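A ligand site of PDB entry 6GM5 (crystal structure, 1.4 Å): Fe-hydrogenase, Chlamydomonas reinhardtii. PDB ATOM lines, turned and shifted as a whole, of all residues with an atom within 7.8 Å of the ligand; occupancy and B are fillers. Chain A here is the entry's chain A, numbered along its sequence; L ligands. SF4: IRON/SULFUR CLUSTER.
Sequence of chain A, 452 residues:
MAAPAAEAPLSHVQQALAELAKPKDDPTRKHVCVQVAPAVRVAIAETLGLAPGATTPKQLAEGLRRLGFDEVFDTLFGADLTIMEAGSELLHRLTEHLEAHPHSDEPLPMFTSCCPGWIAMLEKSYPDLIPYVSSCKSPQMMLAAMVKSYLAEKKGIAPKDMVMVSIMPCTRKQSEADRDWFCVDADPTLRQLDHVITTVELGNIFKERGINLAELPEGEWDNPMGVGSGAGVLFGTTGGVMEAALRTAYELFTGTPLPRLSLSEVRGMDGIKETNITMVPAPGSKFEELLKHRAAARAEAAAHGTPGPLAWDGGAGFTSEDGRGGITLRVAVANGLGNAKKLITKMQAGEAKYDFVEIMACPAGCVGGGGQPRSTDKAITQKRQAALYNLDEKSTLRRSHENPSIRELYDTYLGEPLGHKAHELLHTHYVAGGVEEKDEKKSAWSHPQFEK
SG of Cys 362 is bound to FE2 of the ligand (2.3 Å). FE3 of the ligand is bound by SG of Cys 170, 2.2 Å away. An iron atom (FE1) of the ligand is bound by the side-chain sulfur (SG) of Cys 115. S4 of the ligand lies close to NE of Arg 172 (3.5 Å). The backbone NH of Ala 361 sits close to a sulfur (S3) of the ligand (3.7 Å). An iron atom (FE4) of the ligand is bound by the side-chain sulfur (SG) of Cys 366 (2.3 Å). S3 of the ligand sits close to N of Cys 362, at 3.5 Å.
The backbone carbonyl oxygen of Met 360 lies within hydrogen-bond range of the backbone NH of Gly 336 (2.8 Å). SG of Cys 170 lies close to N of Lys 173 (3.7 Å). The backbone carbonyl oxygen (O) of Cys 114 lies within hydrogen-bond range of the side-chain amino group (NZ) of Lys 173 (2.9 Å). N of Met 360 is in hydrogen-bond range of O of Ala 334, 3.0 Å away. The side-chain amide oxygen (OD1) of Asn 335 lies close to the backbone carbonyl oxygen (O) of Cys 362 (3.2 Å). The backbone NH of Arg 172 lies close to the side-chain sulfur of Cys 170, at 3.3 Å. The side-chain sulfur (SG) of Cys 115 sits close to the backbone NH (N) of Ala 361 (3.3 Å). The side-chain amino group (NZ) of Lys 173 lies within salt-bridge range of the side-chain carboxylate (OE1) of Glu 176, 2.7 Å away.
Pro 116 touches the ligand. CE of Lys 173 touches S2 of the ligand (3.8 Å). CE of Met 360 touches S3 of the ligand, 3.5 Å away. Gly 369 touches the ligand (CA to S1, 3.7 Å). Hydrophobic or aromatic side chains that line the ligand: Pro 116, Met 360 and Ala 361. Within 4 Å of the ligand: Cys 115, Pro 116, Cys 170, Arg 172, Lys 173, Met 360, Ala 361, Cys 362, Cys 366 and Gly 369.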
ATOM      1  N   ALA A  39       1.717  -7.657  -6.946  1.00  0.00           N
ATOM      2  CA  ALA A  39       0.570  -8.023  -7.786  1.00  0.00           C
ATOM      3  C   ALA A  39       0.240  -6.938  -8.806  1.00  0.00           C
ATOM      4  O   ALA A  39      -0.268  -7.240  -9.887  1.00  0.00           O
ATOM      5  CB  ALA A  39      -0.636  -8.336  -6.930  1.00  0.00           C
ATOM      6  N   CYS A 114      -3.355  -9.475   7.175  1.00  0.00           N
ATOM      7  CA  CYS A 114      -2.963  -8.595   6.081  1.00  0.00           C
ATOM      8  C   CYS A 114      -4.094  -8.268   5.116  1.00  0.00           C
ATOM      9  O   CYS A 114      -3.995  -7.290   4.409  1.00  0.00           O
ATOM     10  CB  CYS A 114      -1.807  -9.204   5.309  1.00  0.00           C
ATOM     11  SG  CYS A 114      -2.120 -10.866   4.721  1.00  0.00           S
ATOM     12  N   CYS A 115      -5.141  -9.070   5.085  1.00  0.00           N
ATOM     13  CA  CYS A 115      -6.242  -8.802   4.156  1.00  0.00           C
ATOM     14  C   CYS A 115      -7.337  -7.988   4.840  1.00  0.00           C
ATOM     15  O   CYS A 115      -7.981  -8.476   5.781  1.00  0.00           O
ATOM     16  CB  CYS A 115      -6.824 -10.127   3.619  1.00  0.00           C
ATOM     17  SG  CYS A 115      -8.307  -9.820   2.571  1.00  0.00           S
ATOM     18  N   PRO A 116      -7.606  -6.776   4.329  1.00  0.00           N
ATOM     19  CA  PRO A 116      -8.638  -5.957   5.005  1.00  0.00           C
ATOM     20  C   PRO A 116     -10.052  -6.503   4.824  1.00  0.00           C
ATOM     21  O   PRO A 116     -10.905  -6.167   5.643  1.00  0.00           O
ATOM     22  CB  PRO A 116      -8.503  -4.577   4.347  1.00  0.00           C
ATOM     23  CG  PRO A 116      -7.689  -4.795   3.085  1.00  0.00           C
ATOM     24  CD  PRO A 116      -6.857  -6.027   3.307  1.00  0.00           C
ATOM     25  N   GLY A 117     -10.302  -7.309   3.799  1.00  0.00           N
ATOM     26  CA  GLY A 117     -11.595  -7.981   3.666  1.00  0.00           C
ATOM     27  C   GLY A 117     -11.836  -8.925   4.825  1.00  0.00           C
ATOM     28  O   GLY A 117     -12.951  -9.017   5.379  1.00  0.00           O
ATOM     29  N   TRP A 118     -10.804  -9.674   5.188  1.00  0.00           N
ATOM     30  CA  TRP A 118     -10.863 -10.512   6.386  1.00  0.00           C
ATOM     31  C   TRP A 118     -11.074  -9.673   7.624  1.00  0.00           C
ATOM     32  O   TRP A 118     -11.957  -9.984   8.444  1.00  0.00           O
ATOM     33  CB  TRP A 118      -9.579 -11.336   6.493  1.00  0.00           C
ATOM     34  CG  TRP A 118      -9.263 -11.898   7.857  1.00  0.00           C
ATOM     35  CD1 TRP A 118      -8.061 -11.791   8.502  1.00  0.00           C
ATOM     36  CD2 TRP A 118     -10.126 -12.640   8.751  1.00  0.00           C
ATOM     37  NE1 TRP A 118      -8.116 -12.416   9.718  1.00  0.00           N
ATOM     38  CE2 TRP A 118      -9.380 -12.923   9.906  1.00  0.00           C
ATOM     39  CE3 TRP A 118     -11.468 -13.049   8.690  1.00  0.00           C
ATOM     40  CZ2 TRP A 118      -9.906 -13.656  10.985  1.00  0.00           C
ATOM     41  CZ3 TRP A 118     -11.993 -13.752   9.762  1.00  0.00           C
ATOM     42  CH2 TRP A 118     -11.213 -14.053  10.902  1.00  0.00           C
ATOM     43  N   SER A 138      -0.402  -4.339   7.967  1.00  0.00           N
ATOM     44  CA  SER A 138      -0.064  -4.900   6.660  1.00  0.00           C
ATOM     45  C   SER A 138       1.271  -4.372   6.121  1.00  0.00           C
ATOM     46  O   SER A 138       1.774  -3.373   6.599  1.00  0.00           O
ATOM     47  CB  SER A 138      -1.160  -4.543   5.674  1.00  0.00           C
ATOM     48  OG  SER A 138      -1.086  -3.146   5.413  1.00  0.00           O
ATOM     49  N   MET A 168      -2.102  -0.692  -5.395  1.00  0.00           N
ATOM     50  CA  MET A 168      -2.557  -1.985  -4.878  1.00  0.00           C
ATOM     51  C   MET A 168      -3.469  -2.701  -5.867  1.00  0.00           C
ATOM     52  O   MET A 168      -4.092  -2.070  -6.694  1.00  0.00           O
ATOM     53  CB  MET A 168      -3.310  -1.753  -3.570  1.00  0.00           C
ATOM     54  CG  MET A 168      -2.442  -1.303  -2.431  1.00  0.00           C
ATOM     55  SD  MET A 168      -1.425  -2.711  -1.822  1.00  0.00           S
ATOM     56  CE  MET A 168       0.131  -1.869  -1.709  1.00  0.00           C
ATOM     57  N   PRO A 169      -3.580  -4.027  -5.756  1.00  0.00           N
ATOM     58  CA  PRO A 169      -4.480  -4.800  -6.638  1.00  0.00           C
ATOM     59  C   PRO A 169      -5.885  -4.865  -6.070  1.00  0.00           C
ATOM     60  O   PRO A 169      -6.735  -5.544  -6.623  1.00  0.00           O
ATOM     61  CB  PRO A 169      -3.825  -6.193  -6.622  1.00  0.00           C
ATOM     62  CG  PRO A 169      -3.260  -6.287  -5.219  1.00  0.00           C
ATOM     63  CD  PRO A 169      -2.680  -4.880  -4.973  1.00  0.00           C
ATOM     64  N   CYS A 170      -6.109  -4.099  -5.023  1.00  0.00           N
ATOM     65  CA  CYS A 170      -7.136  -4.357  -4.036  1.00  0.00           C
ATOM     66  C   CYS A 170      -8.034  -3.138  -3.935  1.00  0.00           C
ATOM     67  O   CYS A 170      -7.542  -2.020  -3.783  1.00  0.00           O
ATOM     68  CB  CYS A 170      -6.491  -4.659  -2.671  1.00  0.00           C
ATOM     69  SG  CYS A 170      -7.614  -4.999  -1.481  1.00  0.00           S
ATOM     70  N   THR A 171      -9.349  -3.376  -3.953  1.00  0.00           N
ATOM     71  CA  THR A 171     -10.330  -2.327  -3.773  1.00  0.00           C
ATOM     72  C   THR A 171     -10.654  -2.017  -2.295  1.00  0.00           C
ATOM     73  O   THR A 171     -11.483  -1.149  -2.022  1.00  0.00           O
ATOM     74  CB  THR A 171     -11.638  -2.691  -4.473  1.00  0.00           C
ATOM     75  OG1 THR A 171     -12.040  -3.993  -4.024  1.00  0.00           O
ATOM     76  CG2 THR A 171     -11.426  -2.726  -5.990  1.00  0.00           C
ATOM     77  N   ARG A 172      -9.985  -2.705  -1.375  1.00  0.00           N
ATOM     78  CA  ARG A 172     -10.215  -2.615   0.072  1.00  0.00           C
ATOM     79  C   ARG A 172      -9.041  -1.980   0.832  1.00  0.00           C
ATOM     80  O   ARG A 172      -9.120  -1.702   2.029  1.00  0.00           O
ATOM     81  CB  ARG A 172     -10.475  -4.006   0.651  1.00  0.00           C
ATOM     82  CG  ARG A 172     -11.539  -4.822  -0.109  1.00  0.00           C
ATOM     83  CD  ARG A 172     -11.933  -6.052   0.686  1.00  0.00           C
ATOM     84  NE  ARG A 172     -12.486  -7.152  -0.128  1.00  0.00           N
ATOM     85  CZ  ARG A 172     -13.610  -7.788   0.180  1.00  0.00           C
ATOM     86  NH1 ARG A 172     -14.320  -7.413   1.239  1.00  0.00           N
ATOM     87  NH2 ARG A 172     -14.038  -8.794  -0.585  1.00  0.00           N
ATOM     88  N   LYS A 173      -7.924  -1.731   0.142  1.00  0.00           N
ATOM     89  CA  LYS A 173      -6.741  -1.220   0.840  1.00  0.00           C
ATOM     90  C   LYS A 173      -6.873   0.249   1.262  1.00  0.00           C
ATOM     91  O   LYS A 173      -6.181   0.664   2.185  1.00  0.00           O
ATOM     92  CB  LYS A 173      -5.479  -1.446  -0.032  1.00  0.00           C
ATOM     93  CG  LYS A 173      -4.949  -2.915   0.054  1.00  0.00           C
ATOM     94  CD  LYS A 173      -4.215  -3.204   1.368  1.00  0.00           C
ATOM     95  CE  LYS A 173      -3.998  -4.696   1.550  1.00  0.00           C
ATOM     96  NZ  LYS A 173      -3.287  -4.984   2.829  1.00  0.00           N
ATOM     97  N   GLU A 176      -8.403   0.053   4.698  1.00  0.00           N
ATOM     98  CA  GLU A 176      -7.345  -0.243   5.636  1.00  0.00           C
ATOM     99  C   GLU A 176      -6.566   1.009   6.039  1.00  0.00           C
ATOM    100  O   GLU A 176      -6.363   1.289   7.227  1.00  0.00           O
ATOM    101  CB  GLU A 176      -6.398  -1.260   4.997  1.00  0.00           C
ATOM    102  CG  GLU A 176      -5.268  -1.762   5.885  1.00  0.00           C
ATOM    103  CD  GLU A 176      -4.315  -2.627   5.089  1.00  0.00           C
ATOM    104  OE1 GLU A 176      -4.572  -3.843   4.972  1.00  0.00           O
ATOM    105  OE2 GLU A 176      -3.326  -2.094   4.559  1.00  0.00           O
ATOM    106  N   ALA A 334      -7.191 -20.019   3.681  1.00  0.00           N
ATOM    107  CA  ALA A 334      -8.541 -19.950   3.135  1.00  0.00           C
ATOM    108  C   ALA A 334      -8.600 -18.812   2.134  1.00  0.00           C
ATOM    109  O   ALA A 334      -8.190 -17.700   2.450  1.00  0.00           O
ATOM    110  CB  ALA A 334      -9.556 -19.726   4.217  1.00  0.00           C
ATOM    111  N   ASN A 335      -9.059 -19.092   0.928  1.00  0.00           N
ATOM    112  CA  ASN A 335      -9.276 -18.062  -0.076  1.00  0.00           C
ATOM    113  C   ASN A 335     -10.751 -17.949  -0.368  1.00  0.00           C
ATOM    114  O   ASN A 335     -11.396 -18.934  -0.726  1.00  0.00           O
ATOM    115  CB  ASN A 335      -8.492 -18.366  -1.341  1.00  0.00           C
ATOM    116  CG  ASN A 335      -7.034 -18.038  -1.200  1.00  0.00           C
ATOM    117  OD1 ASN A 335      -6.608 -16.912  -1.453  1.00  0.00           O
ATOM    118  ND2 ASN A 335      -6.255 -18.995  -0.758  1.00  0.00           N
ATOM    119  N   GLY A 336     -11.270 -16.740  -0.204  1.00  0.00           N
ATOM    120  CA  GLY A 336     -12.692 -16.479  -0.345  1.00  0.00           C
ATOM    121  C   GLY A 336     -13.345 -16.395   1.016  1.00  0.00           C
ATOM    122  O   GLY A 336     -13.223 -17.307   1.844  1.00  0.00           O
ATOM    123  N   LEU A 337     -14.095 -15.331   1.265  1.00  0.00           N
ATOM    124  CA  LEU A 337     -14.657 -15.143   2.588  1.00  0.00           C
ATOM    125  C   LEU A 337     -15.736 -16.185   2.905  1.00  0.00           C
ATOM    126  O   LEU A 337     -15.899 -16.551   4.044  1.00  0.00           O
ATOM    127  CB  LEU A 337     -15.230 -13.736   2.748  1.00  0.00           C
ATOM    128  CG  LEU A 337     -14.181 -12.626   2.735  1.00  0.00           C
ATOM    129  CD1 LEU A 337     -14.828 -11.250   2.848  1.00  0.00           C
ATOM    130  CD2 LEU A 337     -13.132 -12.866   3.853  1.00  0.00           C
ATOM    131  N   ILE A 359      -6.421 -15.996   6.126  1.00  0.00           N
ATOM    132  CA  ILE A 359      -7.667 -15.769   5.376  1.00  0.00           C
ATOM    133  C   ILE A 359      -7.482 -14.597   4.419  1.00  0.00           C
ATOM    134  O   ILE A 359      -7.123 -13.505   4.835  1.00  0.00           O
ATOM    135  CB  ILE A 359      -8.847 -15.513   6.305  1.00  0.00           C
ATOM    136  CG1 ILE A 359      -9.087 -16.721   7.195  1.00  0.00           C
ATOM    137  CG2 ILE A 359     -10.118 -15.155   5.485  1.00  0.00           C
ATOM    138  CD1 ILE A 359     -10.100 -16.477   8.310  1.00  0.00           C
ATOM    139  N   MET A 360      -7.713 -14.865   3.131  1.00  0.00           N
ATOM    140  CA  MET A 360      -7.670 -13.849   2.081  1.00  0.00           C
ATOM    141  C   MET A 360      -9.054 -13.792   1.438  1.00  0.00           C
ATOM    142  O   MET A 360      -9.614 -14.831   1.097  1.00  0.00           O
ATOM    143  CB  MET A 360      -6.597 -14.179   1.040  1.00  0.00           C
ATOM    144  CG  MET A 360      -5.198 -14.424   1.612  1.00  0.00           C
ATOM    145  SD  MET A 360      -4.498 -12.992   2.442  1.00  0.00           S
ATOM    146  CE  MET A 360      -4.365 -12.012   1.016  1.00  0.00           C
ATOM    147  N   ALA A 361      -9.582 -12.589   1.225  1.00  0.00           N
ATOM    148  CA  ALA A 361     -10.957 -12.474   0.723  1.00  0.00           C
ATOM    149  C   ALA A 361     -11.093 -12.905  -0.730  1.00  0.00           C
ATOM    150  O   ALA A 361     -12.151 -13.396  -1.126  1.00  0.00           O
ATOM    151  CB  ALA A 361     -11.443 -11.052   0.902  1.00  0.00           C
ATOM    152  N   CYS A 362     -10.062 -12.695  -1.543  1.00  0.00           N
ATOM    153  CA  CYS A 362     -10.160 -13.000  -2.972  1.00  0.00           C
ATOM    154  C   CYS A 362      -9.884 -14.468  -3.227  1.00  0.00           C
ATOM    155  O   CYS A 362      -8.892 -15.031  -2.742  1.00  0.00           O
ATOM    156  CB  CYS A 362      -9.190 -12.114  -3.776  1.00  0.00           C
ATOM    157  SG  CYS A 362      -9.656 -10.348  -3.676  1.00  0.00           S
ATOM    158  N   PRO A 363     -10.789 -15.125  -3.980  1.00  0.00           N
ATOM    159  CA  PRO A 363     -10.610 -16.540  -4.321  1.00  0.00           C
ATOM    160  C   PRO A 363      -9.237 -16.880  -4.864  1.00  0.00           C
ATOM    161  O   PRO A 363      -8.688 -17.937  -4.556  1.00  0.00           O
ATOM    162  CB  PRO A 363     -11.697 -16.764  -5.387  1.00  0.00           C
ATOM    163  CG  PRO A 363     -12.785 -15.852  -4.958  1.00  0.00           C
ATOM    164  CD  PRO A 363     -12.086 -14.603  -4.452  1.00  0.00           C
ATOM    165  N   ALA A 364      -8.649 -15.976  -5.653  1.00  0.00           N
ATOM    166  CA  ALA A 364      -7.318 -16.229  -6.190  1.00  0.00           C
ATOM    167  C   ALA A 364      -6.185 -15.512  -5.432  1.00  0.00           C
ATOM    168  O   ALA A 364      -5.021 -15.536  -5.854  1.00  0.00           O
ATOM    169  CB  ALA A 364      -7.289 -15.852  -7.673  1.00  0.00           C
ATOM    170  N   GLY A 365      -6.527 -14.880  -4.314  1.00  0.00           N
ATOM    171  CA  GLY A 365      -5.545 -14.060  -3.611  1.00  0.00           C
ATOM    172  C   GLY A 365      -5.324 -12.765  -4.364  1.00  0.00           C
ATOM    173  O   GLY A 365      -6.058 -12.450  -5.313  1.00  0.00           O
ATOM    174  N   CYS A 366      -4.311 -12.019  -3.949  1.00  0.00           N
ATOM    175  CA  CYS A 366      -4.158 -10.648  -4.424  1.00  0.00           C
ATOM    176  C   CYS A 366      -3.878 -10.535  -5.910  1.00  0.00           C
ATOM    177  O   CYS A 366      -4.262  -9.531  -6.517  1.00  0.00           O
ATOM    178  CB  CYS A 366      -3.052  -9.944  -3.632  1.00  0.00           C
ATOM    179  SG  CYS A 366      -3.339  -9.816  -1.848  1.00  0.00           S
ATOM    180  N   VAL A 367      -3.278 -11.546  -6.540  1.00  0.00           N
ATOM    181  CA  VAL A 367      -3.138 -11.444  -7.985  1.00  0.00           C
ATOM    182  C   VAL A 367      -4.489 -11.391  -8.675  1.00  0.00           C
ATOM    183  O   VAL A 367      -4.592 -10.878  -9.784  1.00  0.00           O
ATOM    184  CB  VAL A 367      -2.305 -12.581  -8.598  1.00  0.00           C
ATOM    185  CG1 VAL A 367      -0.828 -12.402  -8.232  1.00  0.00           C
ATOM    186  CG2 VAL A 367      -2.852 -13.936  -8.200  1.00  0.00           C
ATOM    187  N   GLY A 368      -5.545 -11.849  -7.986  1.00  0.00           N
ATOM    188  CA  GLY A 368      -6.901 -11.746  -8.518  1.00  0.00           C
ATOM    189  C   GLY A 368      -7.765 -10.728  -7.815  1.00  0.00           C
ATOM    190  O   GLY A 368      -9.004 -10.860  -7.775  1.00  0.00           O
ATOM    191  N   GLY A 369      -7.143  -9.688  -7.252  1.00  0.00           N
ATOM    192  CA  GLY A 369      -7.863  -8.662  -6.516  1.00  0.00           C
ATOM    193  C   GLY A 369      -8.831  -7.841  -7.358  1.00  0.00           C
ATOM    194  O   GLY A 369      -8.755  -7.805  -8.577  1.00  0.00           O
ATOM    195  N   GLY A 370      -9.729  -7.156  -6.676  1.00  0.00           N
ATOM    196  CA  GLY A 370     -10.766  -6.404  -7.350  1.00  0.00           C
ATOM    197  C   GLY A 370     -10.314  -5.193  -8.124  1.00  0.00           C
ATOM    198  O   GLY A 370     -11.098  -4.631  -8.908  1.00  0.00           O
ATOM    199  N   GLY A 371      -9.076  -4.761  -7.893  1.00  0.00           N
ATOM    200  CA  GLY A 371      -8.530  -3.623  -8.615  1.00  0.00           C
ATOM    201  C   GLY A 371      -7.686  -4.029  -9.805  1.00  0.00           C
ATOM    202  O   GLY A 371      -7.077  -3.160 -10.466  1.00  0.00           O
ATOM    203  N   GLN A 372      -7.659  -5.322 -10.107  1.00  0.00           N
ATOM    204  CA  GLN A 372      -6.898  -5.846 -11.241  1.00  0.00           C
ATOM    205  C   GLN A 372      -7.637  -5.751 -12.572  1.00  0.00           C
ATOM    206  O   GLN A 372      -8.878  -5.695 -12.605  1.00  0.00           O
ATOM    207  CB  GLN A 372      -6.508  -7.313 -11.003  1.00  0.00           C
ATOM    208  CG  GLN A 372      -5.635  -7.527  -9.759  1.00  0.00           C
ATOM    209  CD  GLN A 372      -4.212  -7.107  -9.997  1.00  0.00           C
ATOM    210  OE1 GLN A 372      -3.936  -5.955 -10.268  1.00  0.00           O
ATOM    211  NE2 GLN A 372      -3.292  -8.057  -9.902  1.00  0.00           N
HETATM  212 FE1  SF4 L   1      -7.508  -9.299   0.443  1.00  0.00          FE
HETATM  213 FE2  SF4 L   1      -8.152  -9.479  -2.196  1.00  0.00          FE
HETATM  214 FE3  SF4 L   1      -7.200  -7.182  -1.154  1.00  0.00          FE
HETATM  215 FE4  SF4 L   1      -5.538  -9.295  -1.435  1.00  0.00          FE
HETATM  216  S1  SF4 L   1      -6.552  -8.141  -3.120  1.00  0.00           S
HETATM  217  S2  SF4 L   1      -5.666  -7.945   0.361  1.00  0.00           S
HETATM  218  S3  SF4 L   1      -7.009 -11.013  -0.991  1.00  0.00           S
HETATM  219  S4  SF4 L   1      -9.155  -8.181  -0.579  1.00  0.00           S
